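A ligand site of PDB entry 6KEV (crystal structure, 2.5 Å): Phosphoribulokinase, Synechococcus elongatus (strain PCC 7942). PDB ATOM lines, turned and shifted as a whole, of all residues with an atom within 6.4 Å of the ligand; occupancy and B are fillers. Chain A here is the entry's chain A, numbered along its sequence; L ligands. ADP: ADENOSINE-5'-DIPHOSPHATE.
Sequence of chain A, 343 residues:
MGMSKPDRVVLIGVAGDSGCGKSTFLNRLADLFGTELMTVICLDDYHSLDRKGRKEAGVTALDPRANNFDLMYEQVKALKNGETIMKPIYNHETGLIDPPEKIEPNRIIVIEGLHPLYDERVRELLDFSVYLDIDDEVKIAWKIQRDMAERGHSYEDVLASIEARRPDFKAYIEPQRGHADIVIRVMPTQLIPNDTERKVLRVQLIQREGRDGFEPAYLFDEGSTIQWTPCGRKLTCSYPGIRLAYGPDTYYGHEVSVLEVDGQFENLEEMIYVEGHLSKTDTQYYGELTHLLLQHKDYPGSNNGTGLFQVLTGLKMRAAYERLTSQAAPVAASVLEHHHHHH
The backbone NH (N) of Ser 23 is in hydrogen-bond range of an oxygen (O3B) of the ligand. OG of Ser 23 is in hydrogen-bond range of O3B of the ligand (2.5 Å). An oxygen (O2A) of the ligand lies within hydrogen-bond range of the backbone NH (N) of Thr 24, at 3.0 Å. The side-chain hydroxyl (OG1) of Thr 24 sits at hydrogen-bond distance from an oxygen (O2A) of the ligand, at 2.9 Å. The side-chain hydroxyl (OG1) of Thr 306 lies within hydrogen-bond range of a nitrogen (N6) of the ligand (2.9 Å). An oxygen (O2B) of the ligand lies within hydrogen-bond range of the backbone NH (N) of Gly 19. The backbone NH (N) of Lys 22 lies close to an oxygen (O2B) of the ligand. An oxygen (O2B) of the ligand is in hydrogen-bond range of the backbone NH (N) of Cys 20 (3.5 Å).
The side-chain hydroxyl (OG1) of Thr 306 lies within hydrogen-bond range of the side-chain amide oxygen (OD1) of Asn 304 (2.5 Å). The backbone carbonyl oxygen (O) of Gly 21 lies within hydrogen-bond range of the side-chain amide nitrogen (NE2) of Gln 310 (3.3 Å). The side-chain amino group (NZ) of Lys 22 lies within hydrogen-bond range of the backbone carbonyl oxygen (O) of Gly 16. SG of Cys 20 lies close to O of Asp 17 (3.3 Å). The backbone NH (N) of Gly 307 lies within hydrogen-bond range of the backbone carbonyl oxygen (O) of Gly 301.
Residues that only touch the ligand: Gly 21, Ser 18, Trp 142, Asp 17, Gly 301, Pro 300 and Lys 143. Hydrophobic or aromatic side chains within 4 Å of the ligand: Trp 142 and Pro 300. Within 4 Å of the ligand: Asp 17, Ser 18, Gly 19, Cys 20, Gly 21, Lys 22, Ser 23, Thr 24, Trp 142, Lys 143, Pro 300, Gly 301 and Thr 306.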
ATOM      1  N   GLY A  16     -13.204 -16.823  37.041  1.00  0.00           N
ATOM      2  CA  GLY A  16     -12.812 -15.467  36.707  1.00  0.00           C
ATOM      3  C   GLY A  16     -13.783 -14.460  37.285  1.00  0.00           C
ATOM      4  O   GLY A  16     -14.922 -14.764  37.635  1.00  0.00           O
ATOM      5  N   ASP A  17     -13.295 -13.230  37.392  1.00  0.00           N
ATOM      6  CA  ASP A  17     -14.140 -12.110  37.786  1.00  0.00           C
ATOM      7  C   ASP A  17     -14.948 -11.628  36.583  1.00  0.00           C
ATOM      8  O   ASP A  17     -14.770 -12.086  35.452  1.00  0.00           O
ATOM      9  CB  ASP A  17     -13.294 -10.982  38.362  1.00  0.00           C
ATOM     10  CG  ASP A  17     -14.043 -10.153  39.388  1.00  0.00           C
ATOM     11  OD1 ASP A  17     -15.283 -10.059  39.300  1.00  0.00           O
ATOM     12  OD2 ASP A  17     -13.378  -9.596  40.299  1.00  0.00           O
ATOM     13  N   SER A  18     -15.877 -10.714  36.842  1.00  0.00           N
ATOM     14  CA  SER A  18     -16.645 -10.150  35.741  1.00  0.00           C
ATOM     15  C   SER A  18     -15.831  -9.073  35.026  1.00  0.00           C
ATOM     16  O   SER A  18     -14.912  -8.480  35.585  1.00  0.00           O
ATOM     17  CB  SER A  18     -17.977  -9.568  36.243  1.00  0.00           C
ATOM     18  OG  SER A  18     -18.976 -10.576  36.278  1.00  0.00           O
ATOM     19  N   GLY A  19     -16.180  -8.840  33.762  1.00  0.00           N
ATOM     20  CA  GLY A  19     -15.370  -8.012  32.902  1.00  0.00           C
ATOM     21  C   GLY A  19     -14.099  -8.672  32.423  1.00  0.00           C
ATOM     22  O   GLY A  19     -13.255  -7.991  31.824  1.00  0.00           O
ATOM     23  N   CYS A  20     -13.938  -9.971  32.670  1.00  0.00           N
ATOM     24  CA  CYS A  20     -12.762 -10.720  32.257  1.00  0.00           C
ATOM     25  C   CYS A  20     -13.021 -11.589  31.027  1.00  0.00           C
ATOM     26  O   CYS A  20     -12.318 -12.581  30.812  1.00  0.00           O
ATOM     27  CB  CYS A  20     -12.264 -11.593  33.416  1.00  0.00           C
ATOM     28  SG  CYS A  20     -11.844 -10.668  34.917  1.00  0.00           S
ATOM     29  N   GLY A  21     -14.024 -11.242  30.227  1.00  0.00           N
ATOM     30  CA  GLY A  21     -14.330 -12.010  29.032  1.00  0.00           C
ATOM     31  C   GLY A  21     -15.009 -13.331  29.297  1.00  0.00           C
ATOM     32  O   GLY A  21     -14.943 -14.237  28.461  1.00  0.00           O
ATOM     33  N   LYS A  22     -15.692 -13.466  30.439  1.00  0.00           N
ATOM     34  CA  LYS A  22     -16.268 -14.754  30.817  1.00  0.00           C
ATOM     35  C   LYS A  22     -17.546 -15.061  30.035  1.00  0.00           C
ATOM     36  O   LYS A  22     -17.755 -16.200  29.612  1.00  0.00           O
ATOM     37  CB  LYS A  22     -16.519 -14.788  32.319  1.00  0.00           C
ATOM     38  CG  LYS A  22     -16.691 -16.186  32.892  1.00  0.00           C
ATOM     39  CD  LYS A  22     -16.613 -16.138  34.409  1.00  0.00           C
ATOM     40  CE  LYS A  22     -17.581 -15.117  34.984  1.00  0.00           C
ATOM     41  NZ  LYS A  22     -17.533 -15.076  36.473  1.00  0.00           N
ATOM     42  N   SER A  23     -18.414 -14.059  29.842  1.00  0.00           N
ATOM     43  CA  SER A  23     -19.592 -14.280  29.017  1.00  0.00           C
ATOM     44  C   SER A  23     -19.213 -14.498  27.554  1.00  0.00           C
ATOM     45  O   SER A  23     -19.814 -15.323  26.869  1.00  0.00           O
ATOM     46  CB  SER A  23     -20.564 -13.098  29.133  1.00  0.00           C
ATOM     47  OG  SER A  23     -21.055 -12.960  30.463  1.00  0.00           O
ATOM     48  N   THR A  24     -18.211 -13.752  27.076  1.00  0.00           N
ATOM     49  CA  THR A  24     -17.698 -13.976  25.723  1.00  0.00           C
ATOM     50  C   THR A  24     -17.186 -15.397  25.554  1.00  0.00           C
ATOM     51  O   THR A  24     -17.457 -16.051  24.531  1.00  0.00           O
ATOM     52  CB  THR A  24     -16.591 -12.972  25.402  1.00  0.00           C
ATOM     53  OG1 THR A  24     -17.094 -11.635  25.538  1.00  0.00           O
ATOM     54  CG2 THR A  24     -16.066 -13.175  23.990  1.00  0.00           C
ATOM     55  N   PHE A  25     -16.468 -15.898  26.555  1.00  0.00           N
ATOM     56  CA  PHE A  25     -15.928 -17.253  26.501  1.00  0.00           C
ATOM     57  C   PHE A  25     -17.044 -18.295  26.494  1.00  0.00           C
ATOM     58  O   PHE A  25     -16.955 -19.310  25.789  1.00  0.00           O
ATOM     59  CB  PHE A  25     -14.979 -17.485  27.673  1.00  0.00           C
ATOM     60  CG  PHE A  25     -14.398 -18.869  27.731  1.00  0.00           C
ATOM     61  CD1 PHE A  25     -13.391 -19.252  26.860  1.00  0.00           C
ATOM     62  CD2 PHE A  25     -14.859 -19.783  28.671  1.00  0.00           C
ATOM     63  CE1 PHE A  25     -12.861 -20.526  26.924  1.00  0.00           C
ATOM     64  CE2 PHE A  25     -14.320 -21.059  28.732  1.00  0.00           C
ATOM     65  CZ  PHE A  25     -13.329 -21.418  27.855  1.00  0.00           C
ATOM     66  N   LEU A 132      -9.489 -17.318  33.737  1.00  0.00           N
ATOM     67  CA  LEU A 132      -9.288 -16.125  32.927  1.00  0.00           C
ATOM     68  C   LEU A 132      -8.558 -15.089  33.786  1.00  0.00           C
ATOM     69  O   LEU A 132      -9.141 -14.505  34.697  1.00  0.00           O
ATOM     70  CB  LEU A 132     -10.620 -15.586  32.420  1.00  0.00           C
ATOM     71  CG  LEU A 132     -11.529 -16.614  31.735  1.00  0.00           C
ATOM     72  CD1 LEU A 132     -12.850 -15.990  31.345  1.00  0.00           C
ATOM     73  CD2 LEU A 132     -10.852 -17.232  30.517  1.00  0.00           C
ATOM     74  N   TRP A 142      -9.835  -1.861  30.397  1.00  0.00           N
ATOM     75  CA  TRP A 142     -11.114  -2.281  29.828  1.00  0.00           C
ATOM     76  C   TRP A 142     -12.274  -1.546  30.486  1.00  0.00           C
ATOM     77  O   TRP A 142     -13.185  -1.060  29.800  1.00  0.00           O
ATOM     78  CB  TRP A 142     -11.280  -3.796  29.970  1.00  0.00           C
ATOM     79  CG  TRP A 142     -10.424  -4.581  29.017  1.00  0.00           C
ATOM     80  CD1 TRP A 142      -9.623  -4.078  28.033  1.00  0.00           C
ATOM     81  CD2 TRP A 142     -10.291  -6.005  28.963  1.00  0.00           C
ATOM     82  NE1 TRP A 142      -9.000  -5.098  27.368  1.00  0.00           N
ATOM     83  CE2 TRP A 142      -9.385  -6.293  27.920  1.00  0.00           C
ATOM     84  CE3 TRP A 142     -10.838  -7.061  29.690  1.00  0.00           C
ATOM     85  CZ2 TRP A 142      -9.031  -7.597  27.585  1.00  0.00           C
ATOM     86  CZ3 TRP A 142     -10.483  -8.364  29.355  1.00  0.00           C
ATOM     87  CH2 TRP A 142      -9.577  -8.615  28.314  1.00  0.00           C
ATOM     88  N   LYS A 143     -12.274  -1.456  31.817  1.00  0.00           N
ATOM     89  CA  LYS A 143     -13.360  -0.758  32.518  1.00  0.00           C
ATOM     90  C   LYS A 143     -13.358   0.728  32.184  1.00  0.00           C
ATOM     91  O   LYS A 143     -14.430   1.340  32.027  1.00  0.00           O
ATOM     92  CB  LYS A 143     -13.229  -0.957  34.022  1.00  0.00           C
ATOM     93  CG  LYS A 143     -13.344  -2.413  34.467  1.00  0.00           C
ATOM     94  CD  LYS A 143     -14.645  -3.023  33.989  1.00  0.00           C
ATOM     95  CE  LYS A 143     -14.383  -4.314  33.231  1.00  0.00           C
ATOM     96  NZ  LYS A 143     -15.597  -4.768  32.492  1.00  0.00           N
ATOM     97  N   GLN A 145     -12.479   2.071  29.432  1.00  0.00           N
ATOM     98  CA  GLN A 145     -12.975   2.255  28.071  1.00  0.00           C
ATOM     99  C   GLN A 145     -14.446   1.846  27.955  1.00  0.00           C
ATOM    100  O   GLN A 145     -15.144   1.741  28.962  1.00  0.00           O
ATOM    101  CB  GLN A 145     -12.122   1.461  27.075  1.00  0.00           C
ATOM    102  CG  GLN A 145     -10.700   1.962  26.928  1.00  0.00           C
ATOM    103  CD  GLN A 145      -9.869   1.107  26.001  1.00  0.00           C
ATOM    104  OE1 GLN A 145     -10.159  -0.069  25.811  1.00  0.00           O
ATOM    105  NE2 GLN A 145      -8.832   1.701  25.418  1.00  0.00           N
ATOM    106  N   VAL A 186      -4.019 -12.294  30.179  1.00  0.00           N
ATOM    107  CA  VAL A 186      -4.031 -11.117  29.310  1.00  0.00           C
ATOM    108  C   VAL A 186      -3.157 -10.049  29.939  1.00  0.00           C
ATOM    109  O   VAL A 186      -3.318  -9.725  31.124  1.00  0.00           O
ATOM    110  CB  VAL A 186      -5.470 -10.604  29.093  1.00  0.00           C
ATOM    111  CG1 VAL A 186      -5.465  -9.398  28.169  1.00  0.00           C
ATOM    112  CG2 VAL A 186      -6.340 -11.716  28.529  1.00  0.00           C
ATOM    113  N   LYS A 199      -4.922  -1.521  23.991  1.00  0.00           N
ATOM    114  CA  LYS A 199      -5.777  -2.195  23.022  1.00  0.00           C
ATOM    115  C   LYS A 199      -5.060  -3.336  22.318  1.00  0.00           C
ATOM    116  O   LYS A 199      -5.700  -4.299  21.892  1.00  0.00           O
ATOM    117  CB  LYS A 199      -6.330  -1.194  22.001  1.00  0.00           C
ATOM    118  CG  LYS A 199      -7.203  -0.110  22.626  1.00  0.00           C
ATOM    119  CD  LYS A 199      -8.413   0.210  21.758  1.00  0.00           C
ATOM    120  CE  LYS A 199      -9.594  -0.719  22.037  1.00  0.00           C
ATOM    121  NZ  LYS A 199      -9.361  -2.135  21.607  1.00  0.00           N
ATOM    122  N   LEU A 201      -2.631  -6.466  22.895  1.00  0.00           N
ATOM    123  CA  LEU A 201      -2.483  -7.304  24.072  1.00  0.00           C
ATOM    124  C   LEU A 201      -1.476  -8.411  23.836  1.00  0.00           C
ATOM    125  O   LEU A 201      -1.349  -8.949  22.726  1.00  0.00           O
ATOM    126  CB  LEU A 201      -3.835  -7.909  24.484  1.00  0.00           C
ATOM    127  CG  LEU A 201      -4.968  -6.889  24.668  1.00  0.00           C
ATOM    128  CD1 LEU A 201      -6.284  -7.576  25.022  1.00  0.00           C
ATOM    129  CD2 LEU A 201      -4.587  -5.864  25.730  1.00  0.00           C
ATOM    130  N   PRO A 300     -15.660  -9.216  21.648  1.00  0.00           N
ATOM    131  CA  PRO A 300     -14.382  -8.568  21.947  1.00  0.00           C
ATOM    132  C   PRO A 300     -13.237  -9.563  21.912  1.00  0.00           C
ATOM    133  O   PRO A 300     -13.365 -10.709  22.363  1.00  0.00           O
ATOM    134  CB  PRO A 300     -14.591  -7.979  23.350  1.00  0.00           C
ATOM    135  CG  PRO A 300     -15.771  -8.709  23.909  1.00  0.00           C
ATOM    136  CD  PRO A 300     -16.630  -9.049  22.744  1.00  0.00           C
ATOM    137  N   GLY A 301     -12.112  -9.132  21.359  1.00  0.00           N
ATOM    138  CA  GLY A 301     -10.948  -9.977  21.219  1.00  0.00           C
ATOM    139  C   GLY A 301     -10.919 -10.854  19.993  1.00  0.00           C
ATOM    140  O   GLY A 301     -10.054 -11.736  19.905  1.00  0.00           O
ATOM    141  N   SER A 302     -11.829 -10.640  19.037  1.00  0.00           N
ATOM    142  CA  SER A 302     -11.871 -11.445  17.828  1.00  0.00           C
ATOM    143  C   SER A 302     -10.657 -11.251  16.928  1.00  0.00           C
ATOM    144  O   SER A 302     -10.465 -12.057  16.007  1.00  0.00           O
ATOM    145  CB  SER A 302     -13.152 -11.147  17.046  1.00  0.00           C
ATOM    146  OG  SER A 302     -14.297 -11.622  17.740  1.00  0.00           O
ATOM    147  N   ASN A 304      -7.326 -10.612  18.177  1.00  0.00           N
ATOM    148  CA  ASN A 304      -6.063 -10.771  18.897  1.00  0.00           C
ATOM    149  C   ASN A 304      -6.081 -12.114  19.631  1.00  0.00           C
ATOM    150  O   ASN A 304      -6.923 -12.984  19.363  1.00  0.00           O
ATOM    151  CB  ASN A 304      -5.814  -9.579  19.838  1.00  0.00           C
ATOM    152  CG  ASN A 304      -6.892  -9.400  20.876  1.00  0.00           C
ATOM    153  OD1 ASN A 304      -7.101 -10.260  21.731  1.00  0.00           O
ATOM    154  ND2 ASN A 304      -7.591  -8.271  20.820  1.00  0.00           N
ATOM    155  N   THR A 306      -6.802 -13.024  22.669  1.00  0.00           N
ATOM    156  CA  THR A 306      -7.848 -13.368  23.641  1.00  0.00           C
ATOM    157  C   THR A 306      -8.913 -14.236  22.999  1.00  0.00           C
ATOM    158  O   THR A 306      -9.282 -15.290  23.537  1.00  0.00           O
ATOM    159  CB  THR A 306      -8.456 -12.098  24.245  1.00  0.00           C
ATOM    160  OG1 THR A 306      -8.880 -11.216  23.196  1.00  0.00           O
ATOM    161  CG2 THR A 306      -7.442 -11.380  25.114  1.00  0.00           C
ATOM    162  N   GLY A 307      -9.425 -13.838  21.832  1.00  0.00           N
ATOM    163  CA  GLY A 307     -10.370 -14.683  21.128  1.00  0.00           C
ATOM    164  C   GLY A 307      -9.741 -15.959  20.615  1.00  0.00           C
ATOM    165  O   GLY A 307     -10.374 -17.026  20.638  1.00  0.00           O
ATOM    166  N   GLN A 310      -9.296 -18.321  23.597  1.00  0.00           N
ATOM    167  CA  GLN A 310     -10.601 -18.781  24.068  1.00  0.00           C
ATOM    168  C   GLN A 310     -11.104 -19.917  23.203  1.00  0.00           C
ATOM    169  O   GLN A 310     -11.569 -20.946  23.714  1.00  0.00           O
ATOM    170  CB  GLN A 310     -11.597 -17.619  24.075  1.00  0.00           C
ATOM    171  CG  GLN A 310     -11.479 -16.682  25.261  1.00  0.00           C
ATOM    172  CD  GLN A 310     -12.513 -15.580  25.230  1.00  0.00           C
ATOM    173  OE1 GLN A 310     -13.291 -15.465  24.272  1.00  0.00           O
ATOM    174  NE2 GLN A 310     -12.539 -14.748  26.268  1.00  0.00           N
HETATM  175  PB  ADP L   1     -18.123 -10.954  31.923  1.00  0.00           P
HETATM  176  O1B ADP L   1     -19.045  -9.914  32.533  1.00  0.00           O
HETATM  177  O2B ADP L   1     -17.049 -11.496  32.853  1.00  0.00           O
HETATM  178  O3B ADP L   1     -18.830 -12.046  31.134  1.00  0.00           O
HETATM  179  PA  ADP L   1     -17.900 -10.110  29.242  1.00  0.00           P
HETATM  180  O1A ADP L   1     -19.410  -9.951  29.284  1.00  0.00           O
HETATM  181  O2A ADP L   1     -17.287 -11.174  28.377  1.00  0.00           O
HETATM  182  O3A ADP L   1     -17.326 -10.164  30.759  1.00  0.00           O
HETATM  183  O5' ADP L   1     -17.289  -8.680  28.837  1.00  0.00           O
HETATM  184  C5' ADP L   1     -17.635  -7.543  29.615  1.00  0.00           C
HETATM  185  C4' ADP L   1     -16.794  -6.374  29.154  1.00  0.00           C
HETATM  186  O4' ADP L   1     -15.396  -6.652  29.315  1.00  0.00           O
HETATM  187  C3' ADP L   1     -16.995  -6.140  27.666  1.00  0.00           C
HETATM  188  O3' ADP L   1     -18.005  -5.157  27.407  1.00  0.00           O
HETATM  189  C2' ADP L   1     -15.653  -5.654  27.187  1.00  0.00           C
HETATM  190  O2' ADP L   1     -15.682  -4.225  27.178  1.00  0.00           O
HETATM  191  C1' ADP L   1     -14.636  -6.171  28.198  1.00  0.00           C
HETATM  192  N9  ADP L   1     -13.864  -7.282  27.547  1.00  0.00           N
HETATM  193  C8  ADP L   1     -13.987  -8.616  27.773  1.00  0.00           C
HETATM  194  N7  ADP L   1     -13.133  -9.374  26.995  1.00  0.00           N
HETATM  195  C5  ADP L   1     -12.432  -8.502  26.244  1.00  0.00           C
HETATM  196  C6  ADP L   1     -11.359  -8.584  25.199  1.00  0.00           C
HETATM  197  N6  ADP L   1     -10.836  -9.760  24.785  1.00  0.00           N
HETATM  198  N1  ADP L   1     -10.897  -7.434  24.661  1.00  0.00           N
HETATM  199  C2  ADP L   1     -11.392  -6.255  25.052  1.00  0.00           C
HETATM  200  N3  ADP L   1     -12.361  -6.077  25.975  1.00  0.00           N
HETATM  201  C4  ADP L   1     -12.914  -7.146  26.609  1.00  0.00           C
